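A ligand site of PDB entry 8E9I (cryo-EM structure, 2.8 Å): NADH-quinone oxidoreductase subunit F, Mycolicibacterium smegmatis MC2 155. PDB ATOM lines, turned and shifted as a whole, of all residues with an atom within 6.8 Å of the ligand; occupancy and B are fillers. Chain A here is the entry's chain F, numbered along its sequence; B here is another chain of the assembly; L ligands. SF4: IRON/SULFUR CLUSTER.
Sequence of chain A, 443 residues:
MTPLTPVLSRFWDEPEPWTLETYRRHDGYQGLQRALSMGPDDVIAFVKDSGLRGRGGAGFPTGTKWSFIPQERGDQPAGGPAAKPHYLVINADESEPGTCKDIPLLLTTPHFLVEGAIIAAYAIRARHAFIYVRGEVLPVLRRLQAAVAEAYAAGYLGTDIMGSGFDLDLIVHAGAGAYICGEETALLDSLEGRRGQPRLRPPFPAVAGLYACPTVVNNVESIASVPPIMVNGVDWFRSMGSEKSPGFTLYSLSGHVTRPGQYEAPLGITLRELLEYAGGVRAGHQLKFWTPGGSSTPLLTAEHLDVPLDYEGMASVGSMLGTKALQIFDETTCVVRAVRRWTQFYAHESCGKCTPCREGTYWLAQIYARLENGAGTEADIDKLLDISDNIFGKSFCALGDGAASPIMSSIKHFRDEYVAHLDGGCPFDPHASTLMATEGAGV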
ATOM      1  N   ILE A 180      -2.588 -15.088  -4.319  1.00  0.00           N
ATOM      2  CA  ILE A 180      -2.195 -14.071  -5.280  1.00  0.00           C
ATOM      3  C   ILE A 180      -3.194 -12.932  -5.354  1.00  0.00           C
ATOM      4  O   ILE A 180      -2.838 -11.827  -5.761  1.00  0.00           O
ATOM      5  CB  ILE A 180      -1.979 -14.705  -6.668  1.00  0.00           C
ATOM      6  CG1 ILE A 180      -1.520 -13.667  -7.679  1.00  0.00           C
ATOM      7  CG2 ILE A 180      -3.255 -15.363  -7.155  1.00  0.00           C
ATOM      8  CD1 ILE A 180      -0.282 -12.906  -7.264  1.00  0.00           C
ATOM      9  N   GLU A 183      -2.520  -9.130  -4.153  1.00  0.00           N
ATOM     10  CA  GLU A 183      -1.794  -8.082  -4.840  1.00  0.00           C
ATOM     11  C   GLU A 183      -2.746  -7.148  -5.573  1.00  0.00           C
ATOM     12  O   GLU A 183      -3.727  -7.585  -6.174  1.00  0.00           O
ATOM     13  CB  GLU A 183      -0.809  -8.668  -5.842  1.00  0.00           C
ATOM     14  CG  GLU A 183       0.109  -7.628  -6.462  1.00  0.00           C
ATOM     15  CD  GLU A 183       0.603  -8.026  -7.840  1.00  0.00           C
ATOM     16  OE1 GLU A 183       0.800  -9.235  -8.069  1.00  0.00           O
ATOM     17  OE2 GLU A 183       0.782  -7.123  -8.681  1.00  0.00           O
ATOM     18  N   GLN A 197      -5.200 -12.996 -11.448  1.00  0.00           N
ATOM     19  CA  GLN A 197      -3.803 -12.839 -11.827  1.00  0.00           C
ATOM     20  C   GLN A 197      -3.427 -11.370 -11.908  1.00  0.00           C
ATOM     21  O   GLN A 197      -4.256 -10.542 -12.270  1.00  0.00           O
ATOM     22  CB  GLN A 197      -3.530 -13.495 -13.179  1.00  0.00           C
ATOM     23  CG  GLN A 197      -3.745 -14.976 -13.209  1.00  0.00           C
ATOM     24  CD  GLN A 197      -3.082 -15.628 -14.397  1.00  0.00           C
ATOM     25  OE1 GLN A 197      -2.907 -15.000 -15.433  1.00  0.00           O
ATOM     26  NE2 GLN A 197      -2.700 -16.878 -14.242  1.00  0.00           N
ATOM     27  N   PRO A 198      -2.190 -11.029 -11.572  1.00  0.00           N
ATOM     28  CA  PRO A 198      -1.773  -9.621 -11.658  1.00  0.00           C
ATOM     29  C   PRO A 198      -1.780  -9.109 -13.084  1.00  0.00           C
ATOM     30  O   PRO A 198      -1.554  -9.847 -14.042  1.00  0.00           O
ATOM     31  CB  PRO A 198      -0.362  -9.646 -11.083  1.00  0.00           C
ATOM     32  CG  PRO A 198       0.120 -11.016 -11.336  1.00  0.00           C
ATOM     33  CD  PRO A 198      -1.074 -11.906 -11.181  1.00  0.00           C
ATOM     34  N   TYR A 346       4.190 -21.684  -1.998  1.00  0.00           N
ATOM     35  CA  TYR A 346       4.302 -20.794  -3.151  1.00  0.00           C
ATOM     36  C   TYR A 346       3.967 -21.505  -4.444  1.00  0.00           C
ATOM     37  O   TYR A 346       3.333 -20.930  -5.325  1.00  0.00           O
ATOM     38  CB  TYR A 346       5.696 -20.181  -3.195  1.00  0.00           C
ATOM     39  CG  TYR A 346       5.865 -19.076  -2.191  1.00  0.00           C
ATOM     40  CD1 TYR A 346       5.203 -17.880  -2.335  1.00  0.00           C
ATOM     41  CD2 TYR A 346       6.674 -19.243  -1.082  1.00  0.00           C
ATOM     42  CE1 TYR A 346       5.346 -16.872  -1.422  1.00  0.00           C
ATOM     43  CE2 TYR A 346       6.823 -18.241  -0.154  1.00  0.00           C
ATOM     44  CZ  TYR A 346       6.149 -17.056  -0.330  1.00  0.00           C
ATOM     45  OH  TYR A 346       6.304 -16.053   0.590  1.00  0.00           O
ATOM     46  N   GLU A 349       0.214 -21.784  -4.467  1.00  0.00           N
ATOM     47  CA  GLU A 349      -0.476 -20.503  -4.570  1.00  0.00           C
ATOM     48  C   GLU A 349      -0.062 -19.680  -5.772  1.00  0.00           C
ATOM     49  O   GLU A 349      -0.617 -18.602  -5.980  1.00  0.00           O
ATOM     50  CB  GLU A 349      -0.228 -19.692  -3.298  1.00  0.00           C
ATOM     51  N   SER A 350       0.889 -20.155  -6.577  1.00  0.00           N
ATOM     52  CA  SER A 350       1.273 -19.424  -7.774  1.00  0.00           C
ATOM     53  C   SER A 350       0.099 -19.337  -8.739  1.00  0.00           C
ATOM     54  O   SER A 350      -0.673 -20.284  -8.879  1.00  0.00           O
ATOM     55  CB  SER A 350       2.447 -20.120  -8.471  1.00  0.00           C
ATOM     56  OG  SER A 350       3.645 -19.905  -7.753  1.00  0.00           O
ATOM     57  N   CYS A 351      -0.031 -18.185  -9.392  1.00  0.00           N
ATOM     58  CA  CYS A 351      -1.102 -18.051 -10.366  1.00  0.00           C
ATOM     59  C   CYS A 351      -0.743 -18.737 -11.677  1.00  0.00           C
ATOM     60  O   CYS A 351      -1.632 -18.992 -12.496  1.00  0.00           O
ATOM     61  CB  CYS A 351      -1.423 -16.587 -10.611  1.00  0.00           C
ATOM     62  SG  CYS A 351      -0.366 -15.767 -11.795  1.00  0.00           S
ATOM     63  N   GLY A 352       0.529 -19.057 -11.885  1.00  0.00           N
ATOM     64  CA  GLY A 352       0.972 -19.748 -13.080  1.00  0.00           C
ATOM     65  C   GLY A 352       1.223 -18.854 -14.273  1.00  0.00           C
ATOM     66  O   GLY A 352       1.605 -19.368 -15.329  1.00  0.00           O
ATOM     67  N   LYS A 353       1.034 -17.547 -14.135  1.00  0.00           N
ATOM     68  CA  LYS A 353       1.045 -16.683 -15.298  1.00  0.00           C
ATOM     69  C   LYS A 353       2.395 -16.677 -15.993  1.00  0.00           C
ATOM     70  O   LYS A 353       2.467 -16.821 -17.221  1.00  0.00           O
ATOM     71  CB  LYS A 353       0.649 -15.267 -14.898  1.00  0.00           C
ATOM     72  CG  LYS A 353       0.719 -14.268 -16.029  1.00  0.00           C
ATOM     73  CD  LYS A 353       0.050 -12.965 -15.656  1.00  0.00           C
ATOM     74  CE  LYS A 353       0.103 -11.988 -16.801  1.00  0.00           C
ATOM     75  NZ  LYS A 353      -1.066 -11.073 -16.798  1.00  0.00           N
ATOM     76  N   CYS A 354       3.483 -16.530 -15.237  1.00  0.00           N
ATOM     77  CA  CYS A 354       4.798 -16.293 -15.817  1.00  0.00           C
ATOM     78  C   CYS A 354       5.702 -17.495 -15.598  1.00  0.00           C
ATOM     79  O   CYS A 354       5.630 -18.166 -14.571  1.00  0.00           O
ATOM     80  CB  CYS A 354       5.436 -15.031 -15.218  1.00  0.00           C
ATOM     81  SG  CYS A 354       5.872 -15.131 -13.478  1.00  0.00           S
ATOM     82  N   THR A 355       6.559 -17.748 -16.594  1.00  0.00           N
ATOM     83  CA  THR A 355       7.427 -18.920 -16.540  1.00  0.00           C
ATOM     84  C   THR A 355       8.290 -18.952 -15.279  1.00  0.00           C
ATOM     85  O   THR A 355       8.336 -19.997 -14.621  1.00  0.00           O
ATOM     86  CB  THR A 355       8.303 -18.987 -17.789  1.00  0.00           C
ATOM     87  OG1 THR A 355       7.486 -18.959 -18.959  1.00  0.00           O
ATOM     88  CG2 THR A 355       9.132 -20.268 -17.799  1.00  0.00           C
ATOM     89  N   PRO A 356       8.982 -17.874 -14.898  1.00  0.00           N
ATOM     90  CA  PRO A 356       9.874 -17.991 -13.738  1.00  0.00           C
ATOM     91  C   PRO A 356       9.192 -18.544 -12.512  1.00  0.00           C
ATOM     92  O   PRO A 356       9.582 -19.603 -12.024  1.00  0.00           O
ATOM     93  CB  PRO A 356      10.371 -16.548 -13.549  1.00  0.00           C
ATOM     94  CG  PRO A 356      10.270 -15.951 -14.882  1.00  0.00           C
ATOM     95  CD  PRO A 356       9.036 -16.533 -15.489  1.00  0.00           C
ATOM     96  N   CYS A 357       8.157 -17.883 -11.993  1.00  0.00           N
ATOM     97  CA  CYS A 357       7.534 -18.400 -10.782  1.00  0.00           C
ATOM     98  C   CYS A 357       6.923 -19.773 -11.026  1.00  0.00           C
ATOM     99  O   CYS A 357       7.258 -20.740 -10.334  1.00  0.00           O
ATOM    100  CB  CYS A 357       6.487 -17.409 -10.278  1.00  0.00           C
ATOM    101  SG  CYS A 357       5.348 -18.041  -9.027  1.00  0.00           S
ATOM    102  N   ARG A 358       6.083 -19.886 -12.048  1.00  0.00           N
ATOM    103  CA  ARG A 358       5.335 -21.129 -12.270  1.00  0.00           C
ATOM    104  C   ARG A 358       6.262 -22.332 -12.289  1.00  0.00           C
ATOM    105  O   ARG A 358       6.010 -23.337 -11.619  1.00  0.00           O
ATOM    106  CB  ARG A 358       4.555 -21.043 -13.576  1.00  0.00           C
ATOM    107  CG  ARG A 358       3.931 -22.365 -13.992  1.00  0.00           C
ATOM    108  CD  ARG A 358       3.040 -22.248 -15.212  1.00  0.00           C
ATOM    109  NE  ARG A 358       3.321 -21.076 -16.022  1.00  0.00           N
ATOM    110  CZ  ARG A 358       4.169 -21.044 -17.036  1.00  0.00           C
ATOM    111  NH1 ARG A 358       4.883 -22.105 -17.373  1.00  0.00           N
ATOM    112  NH2 ARG A 358       4.313 -19.927 -17.729  1.00  0.00           N
ATOM    113  N   GLU A 359       7.338 -22.248 -13.072  1.00  0.00           N
ATOM    114  CA  GLU A 359       8.230 -23.395 -13.240  1.00  0.00           C
ATOM    115  C   GLU A 359       9.258 -23.499 -12.122  1.00  0.00           C
ATOM    116  O   GLU A 359       9.506 -24.600 -11.613  1.00  0.00           O
ATOM    117  CB  GLU A 359       8.937 -23.302 -14.583  1.00  0.00           C
ATOM    118  N   THR A 361       9.229 -22.435  -9.008  1.00  0.00           N
ATOM    119  CA  THR A 361       8.692 -22.873  -7.718  1.00  0.00           C
ATOM    120  C   THR A 361       8.452 -24.372  -7.719  1.00  0.00           C
ATOM    121  O   THR A 361       8.744 -25.044  -6.728  1.00  0.00           O
ATOM    122  CB  THR A 361       7.398 -22.137  -7.398  1.00  0.00           C
ATOM    123  OG1 THR A 361       6.476 -22.313  -8.482  1.00  0.00           O
ATOM    124  CG2 THR A 361       7.666 -20.665  -7.189  1.00  0.00           C
ATOM    125  N   ILE A 391      14.508 -16.678 -10.507  1.00  0.00           N
ATOM    126  CA  ILE A 391      13.132 -16.281 -10.225  1.00  0.00           C
ATOM    127  C   ILE A 391      13.119 -14.848  -9.700  1.00  0.00           C
ATOM    128  O   ILE A 391      12.371 -14.008 -10.199  1.00  0.00           O
ATOM    129  CB  ILE A 391      12.468 -17.224  -9.204  1.00  0.00           C
ATOM    130  CG1 ILE A 391      12.415 -18.649  -9.760  1.00  0.00           C
ATOM    131  CG2 ILE A 391      11.081 -16.730  -8.857  1.00  0.00           C
ATOM    132  CD1 ILE A 391      11.808 -19.636  -8.816  1.00  0.00           C
ATOM    133  N   SER A 395      10.401 -12.737 -12.220  1.00  0.00           N
ATOM    134  CA  SER A 395       9.003 -13.122 -12.210  1.00  0.00           C
ATOM    135  C   SER A 395       8.108 -11.906 -12.434  1.00  0.00           C
ATOM    136  O   SER A 395       8.470 -10.764 -12.131  1.00  0.00           O
ATOM    137  CB  SER A 395       8.644 -13.799 -10.905  1.00  0.00           C
ATOM    138  OG  SER A 395       8.547 -12.858  -9.858  1.00  0.00           O
ATOM    139  N   PHE A 396       6.912 -12.151 -12.960  1.00  0.00           N
ATOM    140  CA  PHE A 396       6.054 -11.058 -13.392  1.00  0.00           C
ATOM    141  C   PHE A 396       5.666 -10.167 -12.232  1.00  0.00           C
ATOM    142  O   PHE A 396       5.775  -8.938 -12.316  1.00  0.00           O
ATOM    143  CB  PHE A 396       4.818 -11.613 -14.094  1.00  0.00           C
ATOM    144  CG  PHE A 396       3.907 -10.567 -14.640  1.00  0.00           C
ATOM    145  CD1 PHE A 396       4.133 -10.022 -15.882  1.00  0.00           C
ATOM    146  CD2 PHE A 396       2.831 -10.133 -13.912  1.00  0.00           C
ATOM    147  CE1 PHE A 396       3.302  -9.064 -16.386  1.00  0.00           C
ATOM    148  CE2 PHE A 396       1.983  -9.172 -14.415  1.00  0.00           C
ATOM    149  CZ  PHE A 396       2.229  -8.639 -15.656  1.00  0.00           C
ATOM    150  N   CYS A 397       5.233 -10.758 -11.122  1.00  0.00           N
ATOM    151  CA  CYS A 397       4.857  -9.993  -9.945  1.00  0.00           C
ATOM    152  C   CYS A 397       5.816 -10.355  -8.820  1.00  0.00           C
ATOM    153  O   CYS A 397       6.731 -11.153  -8.990  1.00  0.00           O
ATOM    154  CB  CYS A 397       3.410 -10.275  -9.508  1.00  0.00           C
ATOM    155  SG  CYS A 397       3.224 -11.782  -8.567  1.00  0.00           S
ATOM    156  N   ALA A 398       5.570  -9.766  -7.653  1.00  0.00           N
ATOM    157  CA  ALA A 398       6.460  -9.970  -6.529  1.00  0.00           C
ATOM    158  C   ALA A 398       6.272 -11.310  -5.835  1.00  0.00           C
ATOM    159  O   ALA A 398       7.039 -11.614  -4.928  1.00  0.00           O
ATOM    160  CB  ALA A 398       6.291  -8.845  -5.519  1.00  0.00           C
ATOM    161  N   LEU A 399       5.271 -12.110  -6.218  1.00  0.00           N
ATOM    162  CA  LEU A 399       5.126 -13.420  -5.587  1.00  0.00           C
ATOM    163  C   LEU A 399       6.349 -14.284  -5.873  1.00  0.00           C
ATOM    164  O   LEU A 399       6.749 -15.100  -5.022  1.00  0.00           O
ATOM    165  CB  LEU A 399       3.866 -14.113  -6.068  1.00  0.00           C
ATOM    166  CG  LEU A 399       3.493 -15.363  -5.256  1.00  0.00           C
ATOM    167  CD1 LEU A 399       1.991 -15.473  -5.075  1.00  0.00           C
ATOM    168  CD2 LEU A 399       4.045 -16.617  -5.906  1.00  0.00           C
ATOM    169  N   GLY A 400       6.939 -14.149  -7.058  1.00  0.00           N
ATOM    170  CA  GLY A 400       8.175 -14.870  -7.330  1.00  0.00           C
ATOM    171  C   GLY A 400       9.309 -14.424  -6.420  1.00  0.00           C
ATOM    172  O   GLY A 400      10.071 -15.256  -5.909  1.00  0.00           O
ATOM    173  N   ASP A 401       9.438 -13.118  -6.203  1.00  0.00           N
ATOM    174  CA  ASP A 401      10.442 -12.628  -5.266  1.00  0.00           C
ATOM    175  C   ASP A 401      10.190 -13.179  -3.873  1.00  0.00           C
ATOM    176  O   ASP A 401      11.132 -13.563  -3.173  1.00  0.00           O
ATOM    177  CB  ASP A 401      10.431 -11.098  -5.235  1.00  0.00           C
ATOM    178  CG  ASP A 401      10.494 -10.487  -6.614  1.00  0.00           C
ATOM    179  OD1 ASP A 401      10.796 -11.224  -7.582  1.00  0.00           O
ATOM    180  OD2 ASP A 401      10.238  -9.272  -6.738  1.00  0.00           O
ATOM    181  N   ALA B  58       3.958 -12.413 -20.196  1.00  0.00           N
ATOM    182  CA  ALA B  58       3.765 -13.551 -19.309  1.00  0.00           C
ATOM    183  C   ALA B  58       5.028 -14.389 -19.203  1.00  0.00           C
ATOM    184  O   ALA B  58       5.576 -14.583 -18.113  1.00  0.00           O
ATOM    185  CB  ALA B  58       2.605 -14.400 -19.792  1.00  0.00           C
ATOM    186  N   ARG B  60       8.072 -14.026 -19.738  1.00  0.00           N
ATOM    187  CA  ARG B  60       9.298 -13.405 -19.265  1.00  0.00           C
ATOM    188  C   ARG B  60      10.526 -13.857 -20.051  1.00  0.00           C
ATOM    189  O   ARG B  60      11.643 -13.799 -19.541  1.00  0.00           O
ATOM    190  CB  ARG B  60       9.537 -13.693 -17.776  1.00  0.00           C
ATOM    191  CG  ARG B  60       8.353 -13.447 -16.879  1.00  0.00           C
ATOM    192  CD  ARG B  60       7.834 -12.042 -16.997  1.00  0.00           C
ATOM    193  NE  ARG B  60       8.784 -11.066 -16.505  1.00  0.00           N
ATOM    194  CZ  ARG B  60       8.624  -9.757 -16.613  1.00  0.00           C
ATOM    195  NH1 ARG B  60       7.549  -9.232 -17.178  1.00  0.00           N
ATOM    196  NH2 ARG B  60       9.570  -8.946 -16.145  1.00  0.00           N
ATOM    197  N   GLY B 188      -1.268 -22.266 -10.822  1.00  0.00           N
ATOM    198  CA  GLY B 188       0.077 -22.668 -10.460  1.00  0.00           C
ATOM    199  C   GLY B 188       0.711 -23.506 -11.547  1.00  0.00           C
ATOM    200  O   GLY B 188       0.441 -23.332 -12.731  1.00  0.00           O
HETATM  201 FE1  SF4 L   1       4.225 -14.886 -11.958  1.00  0.00          FE
HETATM  202 FE2  SF4 L   1       3.227 -13.728  -9.696  1.00  0.00          FE
HETATM  203 FE3  SF4 L   1       3.958 -16.367  -9.679  1.00  0.00          FE
HETATM  204 FE4  SF4 L   1       1.741 -15.563 -11.054  1.00  0.00          FE
HETATM  205  S1  SF4 L   1       2.064 -15.473  -8.797  1.00  0.00           S
HETATM  206  S2  SF4 L   1       3.358 -16.986 -11.777  1.00  0.00           S
HETATM  207  S3  SF4 L   1       2.406 -13.523 -11.812  1.00  0.00           S
HETATM  208  S4  SF4 L   1       5.317 -14.563  -9.993  1.00  0.00           S
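FE1 of the ligand is bound by SG of Cys 354.
The backbone NH (N) of Gly 400 lies close to a sulfur (S4) of the ligand.
An iron atom (FE3) of the ligand is bound by the side-chain sulfur (SG) of Cys 357, 2.3 Å away.
N of Lys 353 sits close to S2 of the ligand, 3.4 Å away.
The side-chain hydroxyl (OG) of Ser 395 lies close to a sulfur (S4) of the ligand (3.7 Å).
A sulfur (S1) of the ligand sits close to the backbone NH (N) of Cys 351 (3.5 Å).
N of Cys 354 sits close to S2 of the ligand.
FE4 of the ligand is bound by SG of Cys 351 (2.2 Å).
FE2 of the ligand is bound by SG of Cys 397, 2.2 Å away.
N of Gly 352 sits close to S2 of the ligand.
Ile 180 touches the ligand (CD1 to S1, 3.8 Å).
Pro 198 touches the ligand.
Arg 358 touches the ligand.
Phe 396 touches the ligand (CB to S3, 3.8 Å).
CB of Leu 399 touches S1 of the ligand, at 3.5 Å.
Hydrophobic or aromatic side chains within 4 Å of the ligand: Ile 180, Pro 198, Phe 396 and Leu 399.
The backbone NH of Leu 399 sits close to the side-chain sulfur of Cys 397, at 3.1 Å.
O of Cys 357 lies within hydrogen-bond range of OG1 of Thr 361, at 2.6 Å.
The side-chain amino group (NZ) of Lys 353 is in hydrogen-bond range of the backbone carbonyl oxygen (O) of Pro 198, at 3.1 Å.
SG of Cys 397 sits close to OE1 of Glu 183 (3.6 Å).
The backbone carbonyl oxygen (O) of Arg 358 lies within hydrogen-bond range of the side-chain hydroxyl (OG1) of Thr 361, at 3.3 Å.
The backbone carbonyl oxygen (O) of Gly 352 is in hydrogen-bond range of the guanidinium group (NE) of Arg 358, at 2.5 Å.
O of Cys 397 lies within hydrogen-bond range of OG of Ser 395 (2.6 Å).
The side-chain hydroxyl (OG) of Ser 395 sits close to the backbone NH (N) of Gly 400.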
